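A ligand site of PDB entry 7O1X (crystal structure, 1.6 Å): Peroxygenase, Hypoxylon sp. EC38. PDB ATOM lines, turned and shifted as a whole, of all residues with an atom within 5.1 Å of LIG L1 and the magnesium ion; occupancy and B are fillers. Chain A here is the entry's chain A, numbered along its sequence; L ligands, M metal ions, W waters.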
ATOM      1  N   PRO A  38     -31.343 -12.975 -21.123  1.00  0.00           N
ATOM      2  CA  PRO A  38     -31.869 -11.652 -20.807  1.00  0.00           C
ATOM      3  C   PRO A  38     -31.200 -10.520 -21.593  1.00  0.00           C
ATOM      4  O   PRO A  38     -31.533  -9.352 -21.382  1.00  0.00           O
ATOM      5  CB  PRO A  38     -31.580 -11.489 -19.307  1.00  0.00           C
ATOM      6  CG  PRO A  38     -30.628 -12.547 -18.976  1.00  0.00           C
ATOM      7  CD  PRO A  38     -30.386 -13.458 -20.135  1.00  0.00           C
ATOM      8  N   CYS A  39     -30.279 -10.863 -22.475  1.00  0.00           N
ATOM      9  CA  CYS A  39     -29.516  -9.907 -23.312  1.00  0.00           C
ATOM     10  C   CYS A  39     -30.241  -9.720 -24.632  1.00  0.00           C
ATOM     11  O   CYS A  39     -30.373 -10.645 -25.443  1.00  0.00           O
ATOM     12  CB  CYS A  39     -28.134 -10.398 -23.562  1.00  0.00           C
ATOM     13  SG  CYS A  39     -27.232  -9.202 -24.578  1.00  0.00           S
ATOM     14  N   PRO A  40     -30.790  -8.510 -24.907  1.00  0.00           N
ATOM     15  CA  PRO A  40     -31.462  -8.296 -26.186  1.00  0.00           C
ATOM     16  C   PRO A  40     -30.529  -8.473 -27.364  1.00  0.00           C
ATOM     17  O   PRO A  40     -31.017  -8.922 -28.411  1.00  0.00           O
ATOM     18  CB  PRO A  40     -31.916  -6.864 -26.112  1.00  0.00           C
ATOM     19  CG  PRO A  40     -30.947  -6.201 -25.122  1.00  0.00           C
ATOM     20  CD  PRO A  40     -30.627  -7.270 -24.093  1.00  0.00           C
ATOM     21  N   MET A  41     -29.246  -8.207 -27.181  1.00  0.00           N
ATOM     22  CA  MET A  41     -28.327  -8.285 -28.349  1.00  0.00           C
ATOM     23  C   MET A  41     -27.960  -9.734 -28.637  1.00  0.00           C
ATOM     24  O   MET A  41     -27.990 -10.144 -29.808  1.00  0.00           O
ATOM     25  CB  MET A  41     -27.085  -7.410 -28.194  1.00  0.00           C
ATOM     26  CG  MET A  41     -26.148  -7.445 -29.411  1.00  0.00           C
ATOM     27  SD  MET A  41     -27.005  -7.010 -30.964  1.00  0.00           S
ATOM     28  CE  MET A  41     -26.852  -5.221 -30.937  1.00  0.00           C
ATOM     29  N   LEU A  42     -27.549 -10.501 -27.632  1.00  0.00           N
ATOM     30  CA  LEU A  42     -27.265 -11.916 -27.956  1.00  0.00           C
ATOM     31  C   LEU A  42     -28.500 -12.619 -28.507  1.00  0.00           C
ATOM     32  O   LEU A  42     -28.347 -13.453 -29.412  1.00  0.00           O
ATOM     33  CB  LEU A  42     -26.748 -12.642 -26.732  1.00  0.00           C
ATOM     34  CG  LEU A  42     -25.446 -12.115 -26.185  1.00  0.00           C
ATOM     35  CD1 LEU A  42     -24.980 -13.068 -25.088  1.00  0.00           C
ATOM     36  CD2 LEU A  42     -24.385 -11.930 -27.234  1.00  0.00           C
ATOM     37  N   THR A  63     -18.060 -16.698 -30.178  1.00  0.00           N
ATOM     38  CA  THR A  63     -18.384 -15.365 -29.621  1.00  0.00           C
ATOM     39  C   THR A  63     -17.572 -14.303 -30.401  1.00  0.00           C
ATOM     40  O   THR A  63     -18.125 -13.305 -30.894  1.00  0.00           O
ATOM     41  CB  THR A  63     -18.126 -15.323 -28.120  1.00  0.00           C
ATOM     42  OG1 THR A  63     -18.920 -16.344 -27.501  1.00  0.00           O
ATOM     43  CG2 THR A  63     -18.447 -13.962 -27.572  1.00  0.00           C
ATOM     44  N   LEU A  67     -19.670 -11.650 -32.758  1.00  0.00           N
ATOM     45  CA  LEU A  67     -19.698 -10.236 -32.354  1.00  0.00           C
ATOM     46  C   LEU A  67     -18.857  -9.421 -33.337  1.00  0.00           C
ATOM     47  O   LEU A  67     -19.230  -8.284 -33.628  1.00  0.00           O
ATOM     48  CB  LEU A  67     -19.115 -10.074 -30.945  1.00  0.00           C
ATOM     49  CG  LEU A  67     -19.915 -10.655 -29.817  1.00  0.00           C
ATOM     50  CD1 LEU A  67     -19.400 -10.300 -28.458  1.00  0.00           C
ATOM     51  CD2 LEU A  67     -21.311 -10.343 -29.905  1.00  0.00           C
ATOM     52  N   LEU A  71     -21.172  -6.844 -35.548  1.00  0.00           N
ATOM     53  CA  LEU A  71     -21.168  -5.530 -34.827  1.00  0.00           C
ATOM     54  C   LEU A  71     -19.781  -4.916 -34.834  1.00  0.00           C
ATOM     55  O   LEU A  71     -19.637  -3.812 -34.345  1.00  0.00           O
ATOM     56  CB  LEU A  71     -21.635  -5.736 -33.383  1.00  0.00           C
ATOM     57  CG  LEU A  71     -23.029  -6.315 -33.184  1.00  0.00           C
ATOM     58  CD1 LEU A  71     -23.254  -6.594 -31.721  1.00  0.00           C
ATOM     59  CD2 LEU A  71     -24.091  -5.349 -33.728  1.00  0.00           C
ATOM     60  N   ILE A  73     -17.331  -5.824 -32.903  1.00  0.00           N
ATOM     61  CA  ILE A  73     -16.754  -5.875 -31.548  1.00  0.00           C
ATOM     62  C   ILE A  73     -15.358  -6.491 -31.669  1.00  0.00           C
ATOM     63  O   ILE A  73     -15.231  -7.494 -32.375  1.00  0.00           O
ATOM     64  CB  ILE A  73     -17.703  -6.557 -30.560  1.00  0.00           C
ATOM     65  CG1 ILE A  73     -18.964  -5.647 -30.464  1.00  0.00           C
ATOM     66  CG2 ILE A  73     -16.988  -6.737 -29.221  1.00  0.00           C
ATOM     67  CD1 ILE A  73     -19.960  -6.177 -29.649  1.00  0.00           C
ATOM     68  N   LEU A  81     -16.100 -10.663 -22.573  1.00  0.00           N
ATOM     69  CA  LEU A  81     -17.527 -10.944 -22.352  1.00  0.00           C
ATOM     70  C   LEU A  81     -17.752 -12.448 -22.256  1.00  0.00           C
ATOM     71  O   LEU A  81     -18.576 -12.934 -21.422  1.00  0.00           O
ATOM     72  CB  LEU A  81     -18.341 -10.304 -23.481  1.00  0.00           C
ATOM     73  CG  LEU A  81     -18.268  -8.777 -23.512  1.00  0.00           C
ATOM     74  CD1 LEU A  81     -18.875  -8.206 -24.781  1.00  0.00           C
ATOM     75  CD2 LEU A  81     -18.982  -8.272 -22.289  1.00  0.00           C
ATOM     76  N   PHE A  82     -17.083 -13.186 -23.123  1.00  0.00           N
ATOM     77  CA  PHE A  82     -17.196 -14.655 -23.097  1.00  0.00           C
ATOM     78  C   PHE A  82     -16.789 -15.172 -21.711  1.00  0.00           C
ATOM     79  O   PHE A  82     -17.494 -16.055 -21.174  1.00  0.00           O
ATOM     80  CB  PHE A  82     -16.353 -15.323 -24.196  1.00  0.00           C
ATOM     81  CG  PHE A  82     -16.393 -16.818 -24.003  1.00  0.00           C
ATOM     82  CD1 PHE A  82     -17.450 -17.555 -24.551  1.00  0.00           C
ATOM     83  CD2 PHE A  82     -15.442 -17.476 -23.231  1.00  0.00           C
ATOM     84  CE1 PHE A  82     -17.595 -18.897 -24.280  1.00  0.00           C
ATOM     85  CE2 PHE A  82     -15.570 -18.833 -23.014  1.00  0.00           C
ATOM     86  CZ  PHE A  82     -16.665 -19.521 -23.484  1.00  0.00           C
ATOM     87  N   ALA A  85     -19.607 -14.788 -19.414  1.00  0.00           N
ATOM     88  CA  ALA A  85     -20.699 -15.659 -19.842  1.00  0.00           C
ATOM     89  C   ALA A  85     -20.438 -17.078 -19.320  1.00  0.00           C
ATOM     90  O   ALA A  85     -21.382 -17.739 -18.830  1.00  0.00           O
ATOM     91  CB  ALA A  85     -20.880 -15.602 -21.343  1.00  0.00           C
ATOM     92  N   PHE A  97     -21.151 -21.668 -23.163  1.00  0.00           N
ATOM     93  CA  PHE A  97     -22.409 -21.371 -22.431  1.00  0.00           C
ATOM     94  C   PHE A  97     -23.563 -21.459 -23.396  1.00  0.00           C
ATOM     95  O   PHE A  97     -23.400 -21.407 -24.590  1.00  0.00           O
ATOM     96  CB  PHE A  97     -22.374 -20.011 -21.732  1.00  0.00           C
ATOM     97  CG  PHE A  97     -22.399 -18.842 -22.674  1.00  0.00           C
ATOM     98  CD1 PHE A  97     -21.254 -18.496 -23.390  1.00  0.00           C
ATOM     99  CD2 PHE A  97     -23.565 -18.129 -22.909  1.00  0.00           C
ATOM    100  CE1 PHE A  97     -21.258 -17.428 -24.278  1.00  0.00           C
ATOM    101  CE2 PHE A  97     -23.574 -17.055 -23.803  1.00  0.00           C
ATOM    102  CZ  PHE A  97     -22.420 -16.706 -24.508  1.00  0.00           C
ATOM    103  N   LEU A 102     -27.358 -17.483 -18.965  1.00  0.00           N
ATOM    104  CA  LEU A 102     -27.184 -16.043 -18.669  1.00  0.00           C
ATOM    105  C   LEU A 102     -28.329 -15.517 -17.822  1.00  0.00           C
ATOM    106  O   LEU A 102     -28.158 -14.491 -17.187  1.00  0.00           O
ATOM    107  CB  LEU A 102     -27.066 -15.252 -19.967  1.00  0.00           C
ATOM    108  CG  LEU A 102     -25.800 -15.469 -20.809  1.00  0.00           C
ATOM    109  CD1 LEU A 102     -25.896 -14.601 -22.044  1.00  0.00           C
ATOM    110  CD2 LEU A 102     -24.519 -15.237 -20.016  1.00  0.00           C
ATOM    111  N   LEU A 108     -24.719 -12.941 -13.586  1.00  0.00           N
ATOM    112  CA  LEU A 108     -24.594 -11.723 -14.407  1.00  0.00           C
ATOM    113  C   LEU A 108     -25.927 -11.016 -14.441  1.00  0.00           C
ATOM    114  O   LEU A 108     -25.950  -9.770 -14.367  1.00  0.00           O
ATOM    115  CB  LEU A 108     -24.136 -12.056 -15.822  1.00  0.00           C
ATOM    116  CG  LEU A 108     -22.857 -12.865 -15.962  1.00  0.00           C
ATOM    117  CD1 LEU A 108     -22.552 -13.078 -17.447  1.00  0.00           C
ATOM    118  CD2 LEU A 108     -21.685 -12.209 -15.224  1.00  0.00           C
ATOM    119  N   GLU A 109     -27.012 -11.760 -14.542  1.00  0.00           N
ATOM    120  CA  GLU A 109     -28.352 -11.140 -14.590  1.00  0.00           C
ATOM    121  C   GLU A 109     -28.568 -10.366 -13.292  1.00  0.00           C
ATOM    122  O   GLU A 109     -28.188 -10.858 -12.181  1.00  0.00           O
ATOM    123  CB  GLU A 109     -29.424 -12.178 -14.887  1.00  0.00           C
ATOM    124  CG  GLU A 109     -30.806 -11.602 -15.134  1.00  0.00           C
ATOM    125  CD  GLU A 109     -31.608 -11.147 -13.903  1.00  0.00           C
ATOM    126  OE1 GLU A 109     -31.577 -11.907 -12.904  1.00  0.00           O
ATOM    127  OE2 GLU A 109     -32.191 -10.032 -13.926  1.00  0.00           O
ATOM    128  N   HIS A 110     -29.162  -9.203 -13.418  1.00  0.00           N
ATOM    129  CA  HIS A 110     -29.353  -8.277 -12.263  1.00  0.00           C
ATOM    130  C   HIS A 110     -30.694  -7.544 -12.317  1.00  0.00           C
ATOM    131  O   HIS A 110     -31.356  -7.419 -13.371  1.00  0.00           O
ATOM    132  CB  HIS A 110     -28.207  -7.252 -12.190  1.00  0.00           C
ATOM    133  CG  HIS A 110     -28.066  -6.490 -13.454  1.00  0.00           C
ATOM    134  ND1 HIS A 110     -28.897  -5.409 -13.749  1.00  0.00           N
ATOM    135  CD2 HIS A 110     -27.168  -6.627 -14.494  1.00  0.00           C
ATOM    136  CE1 HIS A 110     -28.543  -4.972 -14.933  1.00  0.00           C
ATOM    137  NE2 HIS A 110     -27.520  -5.677 -15.411  1.00  0.00           N
ATOM    138  N   ASP A 111     -31.134  -7.146 -11.129  1.00  0.00           N
ATOM    139  CA  ASP A 111     -32.290  -6.259 -10.989  1.00  0.00           C
ATOM    140  C   ASP A 111     -32.084  -4.942 -11.722  1.00  0.00           C
ATOM    141  O   ASP A 111     -30.948  -4.575 -12.149  1.00  0.00           O
ATOM    142  CB  ASP A 111     -32.584  -6.031  -9.520  1.00  0.00           C
ATOM    143  CG  ASP A 111     -32.974  -7.273  -8.722  1.00  0.00           C
ATOM    144  OD1 ASP A 111     -33.474  -8.267  -9.339  1.00  0.00           O
ATOM    145  OD2 ASP A 111     -32.759  -7.242  -7.461  1.00  0.00           O
ATOM    146  N   SER A 113     -33.143  -3.946 -14.625  1.00  0.00           N
ATOM    147  CA  SER A 113     -32.978  -4.043 -16.068  1.00  0.00           C
ATOM    148  C   SER A 113     -33.933  -3.054 -16.744  1.00  0.00           C
ATOM    149  O   SER A 113     -34.955  -2.672 -16.167  1.00  0.00           O
ATOM    150  CB  SER A 113     -33.199  -5.459 -16.618  1.00  0.00           C
ATOM    151  OG  SER A 113     -32.310  -6.403 -16.058  1.00  0.00           O
ATOM    152  N   LEU A 114     -33.525  -2.609 -17.944  1.00  0.00           N
ATOM    153  CA  LEU A 114     -34.284  -1.589 -18.734  1.00  0.00           C
ATOM    154  C   LEU A 114     -35.550  -2.200 -19.336  1.00  0.00           C
ATOM    155  O   LEU A 114     -36.475  -1.425 -19.666  1.00  0.00           O
ATOM    156  CB  LEU A 114     -33.391  -1.055 -19.832  1.00  0.00           C
ATOM    157  CG  LEU A 114     -32.077  -0.437 -19.350  1.00  0.00           C
ATOM    158  CD1 LEU A 114     -31.243  -0.021 -20.543  1.00  0.00           C
ATOM    159  CD2 LEU A 114     -32.280   0.734 -18.437  1.00  0.00           C
ATOM    160  N   SER A 115     -35.535  -3.514 -19.619  1.00  0.00           N
ATOM    161  CA  SER A 115     -36.630  -4.094 -20.472  1.00  0.00           C
ATOM    162  C   SER A 115     -37.127  -5.426 -19.871  1.00  0.00           C
ATOM    163  O   SER A 115     -37.922  -6.063 -20.533  1.00  0.00           O
ATOM    164  CB  SER A 115     -36.139  -4.335 -21.903  1.00  0.00           C
ATOM    165  OG  SER A 115     -35.124  -5.389 -21.931  1.00  0.00           O
ATOM    166  N   ARG A 116     -36.569  -5.858 -18.749  1.00  0.00           N
ATOM    167  CA  ARG A 116     -36.920  -7.107 -18.040  1.00  0.00           C
ATOM    168  C   ARG A 116     -37.403  -6.751 -16.646  1.00  0.00           C
ATOM    169  O   ARG A 116     -36.897  -5.788 -16.068  1.00  0.00           O
ATOM    170  CB  ARG A 116     -35.774  -8.112 -17.907  1.00  0.00           C
ATOM    171  CG  ARG A 116     -35.569  -8.970 -19.153  1.00  0.00           C
ATOM    172  CD  ARG A 116     -35.373  -8.268 -20.468  1.00  0.00           C
ATOM    173  NE  ARG A 116     -35.135  -9.276 -21.486  1.00  0.00           N
ATOM    174  CZ  ARG A 116     -35.149  -9.091 -22.799  1.00  0.00           C
ATOM    175  NH1 ARG A 116     -35.366  -7.868 -23.266  1.00  0.00           N
ATOM    176  NH2 ARG A 116     -35.013 -10.139 -23.654  1.00  0.00           N
ATOM    177  N   GLN A 117     -38.378  -7.511 -16.152  1.00  0.00           N
ATOM    178  CA  GLN A 117     -38.715  -7.401 -14.722  1.00  0.00           C
ATOM    179  C   GLN A 117     -37.588  -8.004 -13.886  1.00  0.00           C
ATOM    180  O   GLN A 117     -36.895  -8.911 -14.298  1.00  0.00           O
ATOM    181  CB  GLN A 117     -40.105  -7.990 -14.464  1.00  0.00           C
ATOM    182  CG  GLN A 117     -40.136  -9.474 -14.527  1.00  0.00           C
ATOM    183  CD  GLN A 117     -41.528 -10.036 -14.771  1.00  0.00           C
ATOM    184  OE1 GLN A 117     -42.566  -9.523 -14.241  1.00  0.00           O
ATOM    185  NE2 GLN A 117     -41.549 -11.125 -15.531  1.00  0.00           N
ATOM    186  N   ALA A 124     -36.967 -13.105 -15.395  1.00  0.00           N
ATOM    187  CA  ALA A 124     -36.119 -11.929 -15.710  1.00  0.00           C
ATOM    188  C   ALA A 124     -35.403 -12.118 -17.044  1.00  0.00           C
ATOM    189  O   ALA A 124     -34.451 -11.396 -17.312  1.00  0.00           O
ATOM    190  CB  ALA A 124     -35.140 -11.694 -14.595  1.00  0.00           C
ATOM    191  N   PHE A 176     -22.084  -4.149 -14.918  1.00  0.00           N
ATOM    192  CA  PHE A 176     -22.880  -4.650 -16.060  1.00  0.00           C
ATOM    193  C   PHE A 176     -23.928  -3.580 -16.399  1.00  0.00           C
ATOM    194  O   PHE A 176     -24.055  -3.250 -17.542  1.00  0.00           O
ATOM    195  CB  PHE A 176     -23.509  -6.025 -15.814  1.00  0.00           C
ATOM    196  CG  PHE A 176     -22.751  -7.145 -16.433  1.00  0.00           C
ATOM    197  CD1 PHE A 176     -21.433  -7.374 -16.022  1.00  0.00           C
ATOM    198  CD2 PHE A 176     -23.339  -7.987 -17.416  1.00  0.00           C
ATOM    199  CE1 PHE A 176     -20.724  -8.414 -16.611  1.00  0.00           C
ATOM    200  CE2 PHE A 176     -22.593  -9.020 -17.983  1.00  0.00           C
ATOM    201  CZ  PHE A 176     -21.307  -9.223 -17.545  1.00  0.00           C
ATOM    202  N   GLU A 180     -24.200  -1.825 -19.952  1.00  0.00           N
ATOM    203  CA  GLU A 180     -25.274  -2.194 -20.919  1.00  0.00           C
ATOM    204  C   GLU A 180     -25.809  -0.909 -21.551  1.00  0.00           C
ATOM    205  O   GLU A 180     -26.086  -0.894 -22.730  1.00  0.00           O
ATOM    206  CB  GLU A 180     -26.378  -2.929 -20.199  1.00  0.00           C
ATOM    207  CG  GLU A 180     -25.952  -4.284 -19.665  1.00  0.00           C
ATOM    208  CD  GLU A 180     -26.609  -4.740 -18.345  1.00  0.00           C
ATOM    209  OE1 GLU A 180     -27.556  -4.103 -17.896  1.00  0.00           O
ATOM    210  OE2 GLU A 180     -26.096  -5.722 -17.735  1.00  0.00           O
ATOM    211  N   ALA A 183     -23.283   0.225 -23.957  1.00  0.00           N
ATOM    212  CA  ALA A 183     -23.257  -0.665 -25.128  1.00  0.00           C
ATOM    213  C   ALA A 183     -24.310  -0.253 -26.175  1.00  0.00           C
ATOM    214  O   ALA A 183     -23.996  -0.189 -27.360  1.00  0.00           O
ATOM    215  CB  ALA A 183     -23.472  -2.105 -24.681  1.00  0.00           C
ATOM    216  N   TYR A 184     -25.541  -0.019 -25.759  1.00  0.00           N
ATOM    217  CA  TYR A 184     -26.588   0.303 -26.779  1.00  0.00           C
ATOM    218  C   TYR A 184     -26.227   1.597 -27.489  1.00  0.00           C
ATOM    219  O   TYR A 184     -26.481   1.725 -28.649  1.00  0.00           O
ATOM    220  CB  TYR A 184     -28.015   0.165 -26.279  1.00  0.00           C
ATOM    221  CG  TYR A 184     -28.537   1.226 -25.365  1.00  0.00           C
ATOM    222  CD1 TYR A 184     -28.882   2.476 -25.843  1.00  0.00           C
ATOM    223  CD2 TYR A 184     -28.903   0.911 -24.056  1.00  0.00           C
ATOM    224  CE1 TYR A 184     -29.433   3.419 -24.982  1.00  0.00           C
ATOM    225  CE2 TYR A 184     -29.471   1.836 -23.214  1.00  0.00           C
ATOM    226  CZ  TYR A 184     -29.755   3.104 -23.687  1.00  0.00           C
ATOM    227  OH  TYR A 184     -30.305   4.044 -22.867  1.00  0.00           O
ATOM    228  N   ILE A 187     -22.479   0.659 -29.487  1.00  0.00           N
ATOM    229  CA  ILE A 187     -22.469  -0.468 -30.430  1.00  0.00           C
ATOM    230  C   ILE A 187     -23.544  -0.277 -31.503  1.00  0.00           C
ATOM    231  O   ILE A 187     -23.279  -0.580 -32.671  1.00  0.00           O
ATOM    232  CB  ILE A 187     -22.571  -1.782 -29.610  1.00  0.00           C
ATOM    233  CG1 ILE A 187     -21.251  -2.005 -28.846  1.00  0.00           C
ATOM    234  CG2 ILE A 187     -22.912  -2.903 -30.559  1.00  0.00           C
ATOM    235  CD1 ILE A 187     -21.203  -3.107 -27.750  1.00  0.00           C
ATOM    236  N   LEU A 204     -34.520  -2.822 -31.596  1.00  0.00           N
ATOM    237  CA  LEU A 204     -33.722  -3.943 -31.085  1.00  0.00           C
ATOM    238  C   LEU A 204     -34.465  -4.606 -29.922  1.00  0.00           C
ATOM    239  O   LEU A 204     -34.568  -5.820 -29.877  1.00  0.00           O
ATOM    240  CB  LEU A 204     -32.372  -3.411 -30.659  1.00  0.00           C
ATOM    241  CG  LEU A 204     -31.436  -4.540 -30.182  1.00  0.00           C
ATOM    242  CD1 LEU A 204     -30.757  -5.191 -31.355  1.00  0.00           C
ATOM    243  CD2 LEU A 204     -30.392  -4.059 -29.193  1.00  0.00           C
ATOM    244  N   PHE A 205     -34.852  -3.833 -28.930  1.00  0.00           N
ATOM    245  CA  PHE A 205     -35.510  -4.407 -27.733  1.00  0.00           C
ATOM    246  C   PHE A 205     -36.826  -5.094 -28.083  1.00  0.00           C
ATOM    247  O   PHE A 205     -37.091  -6.208 -27.585  1.00  0.00           O
ATOM    248  CB  PHE A 205     -35.692  -3.350 -26.670  1.00  0.00           C
ATOM    249  CG  PHE A 205     -34.502  -3.050 -25.833  1.00  0.00           C
ATOM    250  CD1 PHE A 205     -33.582  -2.094 -26.168  1.00  0.00           C
ATOM    251  CD2 PHE A 205     -34.314  -3.726 -24.646  1.00  0.00           C
ATOM    252  CE1 PHE A 205     -32.539  -1.788 -25.306  1.00  0.00           C
ATOM    253  CE2 PHE A 205     -33.237  -3.475 -23.826  1.00  0.00           C
ATOM    254  CZ  PHE A 205     -32.392  -2.428 -24.128  1.00  0.00           C
HETATM  255  C1  LIG L   1     -28.121  -7.224 -20.905  1.00  0.00           C
HETATM  256  C2  LIG L   1     -24.727 -10.591 -21.251  1.00  0.00           C
HETATM  257  C3  LIG L   1     -23.274  -8.709 -25.448  1.00  0.00           C
HETATM  258  C4  LIG L   1     -26.458  -5.063 -24.914  1.00  0.00           C
HETATM  259  C5  LIG L   1     -27.375  -8.355 -20.697  1.00  0.00           C
HETATM  260  C6  LIG L   1     -27.574  -9.263 -19.613  1.00  0.00           C
HETATM  261  C7  LIG L   1     -26.629 -10.224 -19.686  1.00  0.00           C
HETATM  262  C8  LIG L   1     -25.837  -9.912 -20.832  1.00  0.00           C
HETATM  263  C9  LIG L   1     -26.344 -11.355 -18.739  1.00  0.00           C
HETATM  264  C10 LIG L   1     -28.661  -9.159 -18.579  1.00  0.00           C
HETATM  265  C11 LIG L   1     -28.387  -8.132 -17.508  1.00  0.00           C
HETATM  266  C12 LIG L   1     -29.648  -7.735 -16.869  1.00  0.00           C
HETATM  267  O1  LIG L   1     -30.265  -6.748 -17.467  1.00  0.00           O
HETATM  268  O2  LIG L   1     -30.216  -8.291 -15.918  1.00  0.00           O
HETATM  269  C13 LIG L   1     -23.999 -10.298 -22.419  1.00  0.00           C
HETATM  270  C14 LIG L   1     -22.879 -11.094 -22.880  1.00  0.00           C
HETATM  271  C15 LIG L   1     -22.498 -10.630 -24.049  1.00  0.00           C
HETATM  272  C16 LIG L   1     -23.380  -9.469 -24.331  1.00  0.00           C
HETATM  273  C17 LIG L   1     -22.280 -12.268 -22.148  1.00  0.00           C
HETATM  274  C18 LIG L   1     -21.462 -11.079 -24.968  1.00  0.00           C
HETATM  275  C19 LIG L   1     -20.881 -12.299 -24.998  1.00  0.00           C
HETATM  276  C20 LIG L   1     -24.012  -7.523 -25.699  1.00  0.00           C
HETATM  277  C21 LIG L   1     -23.870  -6.609 -26.767  1.00  0.00           C
HETATM  278  C22 LIG L   1     -24.735  -5.607 -26.613  1.00  0.00           C
HETATM  279  C23 LIG L   1     -25.467  -5.889 -25.392  1.00  0.00           C
HETATM  280  C24 LIG L   1     -22.813  -6.830 -27.855  1.00  0.00           C
HETATM  281  C25 LIG L   1     -24.833  -4.530 -27.551  1.00  0.00           C
HETATM  282  C26 LIG L   1     -25.762  -3.676 -27.793  1.00  0.00           C
HETATM  283  C27 LIG L   1     -27.154  -5.378 -23.732  1.00  0.00           C
HETATM  284  C28 LIG L   1     -28.178  -4.502 -23.183  1.00  0.00           C
HETATM  285  C29 LIG L   1     -28.688  -5.057 -22.078  1.00  0.00           C
HETATM  286  C30 LIG L   1     -27.906  -6.347 -21.947  1.00  0.00           C
HETATM  287  C31 LIG L   1     -28.571  -3.182 -23.772  1.00  0.00           C
HETATM  288  C32 LIG L   1     -29.662  -4.556 -21.080  1.00  0.00           C
HETATM  289  C33 LIG L   1     -31.038  -5.247 -21.167  1.00  0.00           C
HETATM  290  C34 LIG L   1     -32.026  -4.662 -20.176  1.00  0.00           C
HETATM  291  O3  LIG L   1     -33.229  -4.920 -20.237  1.00  0.00           O
HETATM  292  O4  LIG L   1     -31.578  -3.899 -19.267  1.00  0.00           O
HETATM  293  N1  LIG L   1     -26.345  -8.757 -21.449  1.00  0.00           N
HETATM  294  N2  LIG L   1     -24.225  -9.338 -23.282  1.00  0.00           N
HETATM  295  N3  LIG L   1     -24.975  -7.117 -24.853  1.00  0.00           N
HETATM  296  N4  LIG L   1     -26.975  -6.468 -22.953  1.00  0.00           N
HETATM  297 FE1  LIG L   1     -25.720  -7.966 -23.205  1.00  0.00          FE
HETATM  298  N1  LG2 L   2     -22.466  -5.933 -21.072  1.00  0.00           N
HETATM  299  C1  LG2 L   2     -23.313  -6.994 -21.151  1.00  0.00           C
HETATM  300  N2  LG2 L   2     -24.204  -6.658 -22.130  1.00  0.00           N
HETATM  301  C2  LG2 L   2     -23.783  -5.367 -22.543  1.00  0.00           C
HETATM  302  C3  LG2 L   2     -22.611  -4.974 -21.954  1.00  0.00           C
HETATM  303  C4  LG2 L   2     -21.446  -5.897 -20.214  1.00  0.00           C
HETATM  304  C5  LG2 L   2     -21.162  -4.703 -19.510  1.00  0.00           C
HETATM  305  C6  LG2 L   2     -20.052  -4.612 -18.603  1.00  0.00           C
HETATM  306  C7  LG2 L   2     -19.237  -5.733 -18.313  1.00  0.00           C
HETATM  307  C8  LG2 L   2     -19.523  -6.940 -18.991  1.00  0.00           C
HETATM  308  C9  LG2 L   2     -20.641  -7.011 -19.905  1.00  0.00           C
HETATM  309 MG    MG M   1     -32.173  -8.254 -15.081  1.00  0.00          MG
HETATM  310  O   HOH W   1     -32.876  -9.238 -16.818  1.00  0.00           O
HETATM  311  O   HOH W   2     -34.116  -7.983 -14.306  1.00  0.00           O
HETATM  312  O   HOH W   3     -32.308  -8.032 -19.138  1.00  0.00           O
HETATM  313  O   HOH W   4     -29.487  -2.513 -18.239  1.00  0.00           O
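A ring nitrogen (NE2) of His 110 lies within hydrogen-bond range of the side-chain carboxylate of Glu 180, at 2.7 Å. The side-chain sulfur of Cys 39 lies close to the backbone NH of Met 41 (3.4 Å). The side-chain sulfur (SG) of Cys 39 sits close to the backbone NH (N) of Leu 42 (3.3 Å). OG of Ser 115 is in hydrogen-bond range of NH1 of Arg 116 (2.8 Å). N of Ile 73 lies within hydrogen-bond range of O of Leu 67 (3.2 Å).
The backbone carbonyl oxygen (O) of His 110 binds the magnesium ion. The magnesium ion is bound by OG of Ser 113, 2.1 Å away. Water W2 is bound to the magnesium ion, at 2.1 Å. Water W1 is bound to the magnesium ion. OE2 of Glu 109 is bound to the magnesium ion, 2.1 Å away. An oxygen (O2) of LIG L1 binds the magnesium ion.
N2 of LG2 L2 is bound to FE1 of LIG L1 (2.3 Å).
Residues that only touch LIG L1: Glu 180 (3.3 Å), Met 41 (3.4 Å), Ile 73 (3.4 Å), Leu 81 (3.5 Å), Pro 40 (3.6 Å), Leu 42 (3.6 Å), Ala 85 (3.7 Å), Leu 108 (3.7 Å), Arg 116 (3.8 Å), Pro 38 (3.8 Å), Phe 205 (3.9 Å), Leu 71 (3.9 Å), Ile 187 (3.9 Å), Thr 63 (3.9 Å), Ala 183 (3.9 Å) and Leu 102 (3.9 Å). Within 4 Å of LIG L1: Pro 38, Cys 39, Pro 40, Met 41, Leu 42, Thr 63, Leu 71, Ile 73, Leu 81, Ala 85, Leu 102, Leu 108, Glu 109, His 110, Ser 113, Leu 114, Ser 115, Arg 116, Glu 180, Ala 183, Ile 187 and Phe 205.
Water W4 lies within hydrogen-bond range of OE1 of Glu 180 and O4 of LIG L1. Water W3 bridges O of Pro 38 (2.7 Å) and O1 of LIG L1 (2.9 Å).
N of His 110 lies close to O2 of LIG L1, 2.9 Å away. FE1 of LIG L1 is bound by SG of Cys 39 (2.4 Å). An oxygen (O3) of LIG L1 lies within hydrogen-bond range of the backbone NH (N) of Ser 115. An oxygen (O3) of LIG L1 sits at hydrogen-bond distance from the side-chain hydroxyl (OG) of Ser 115, 2.6 Å away. An oxygen (O4) of LIG L1 is in hydrogen-bond range of the backbone NH (N) of Leu 114, 2.7 Å away.
The nearest printed residue that does not touch the magnesium ion is Asp 111 (4.2 Å).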
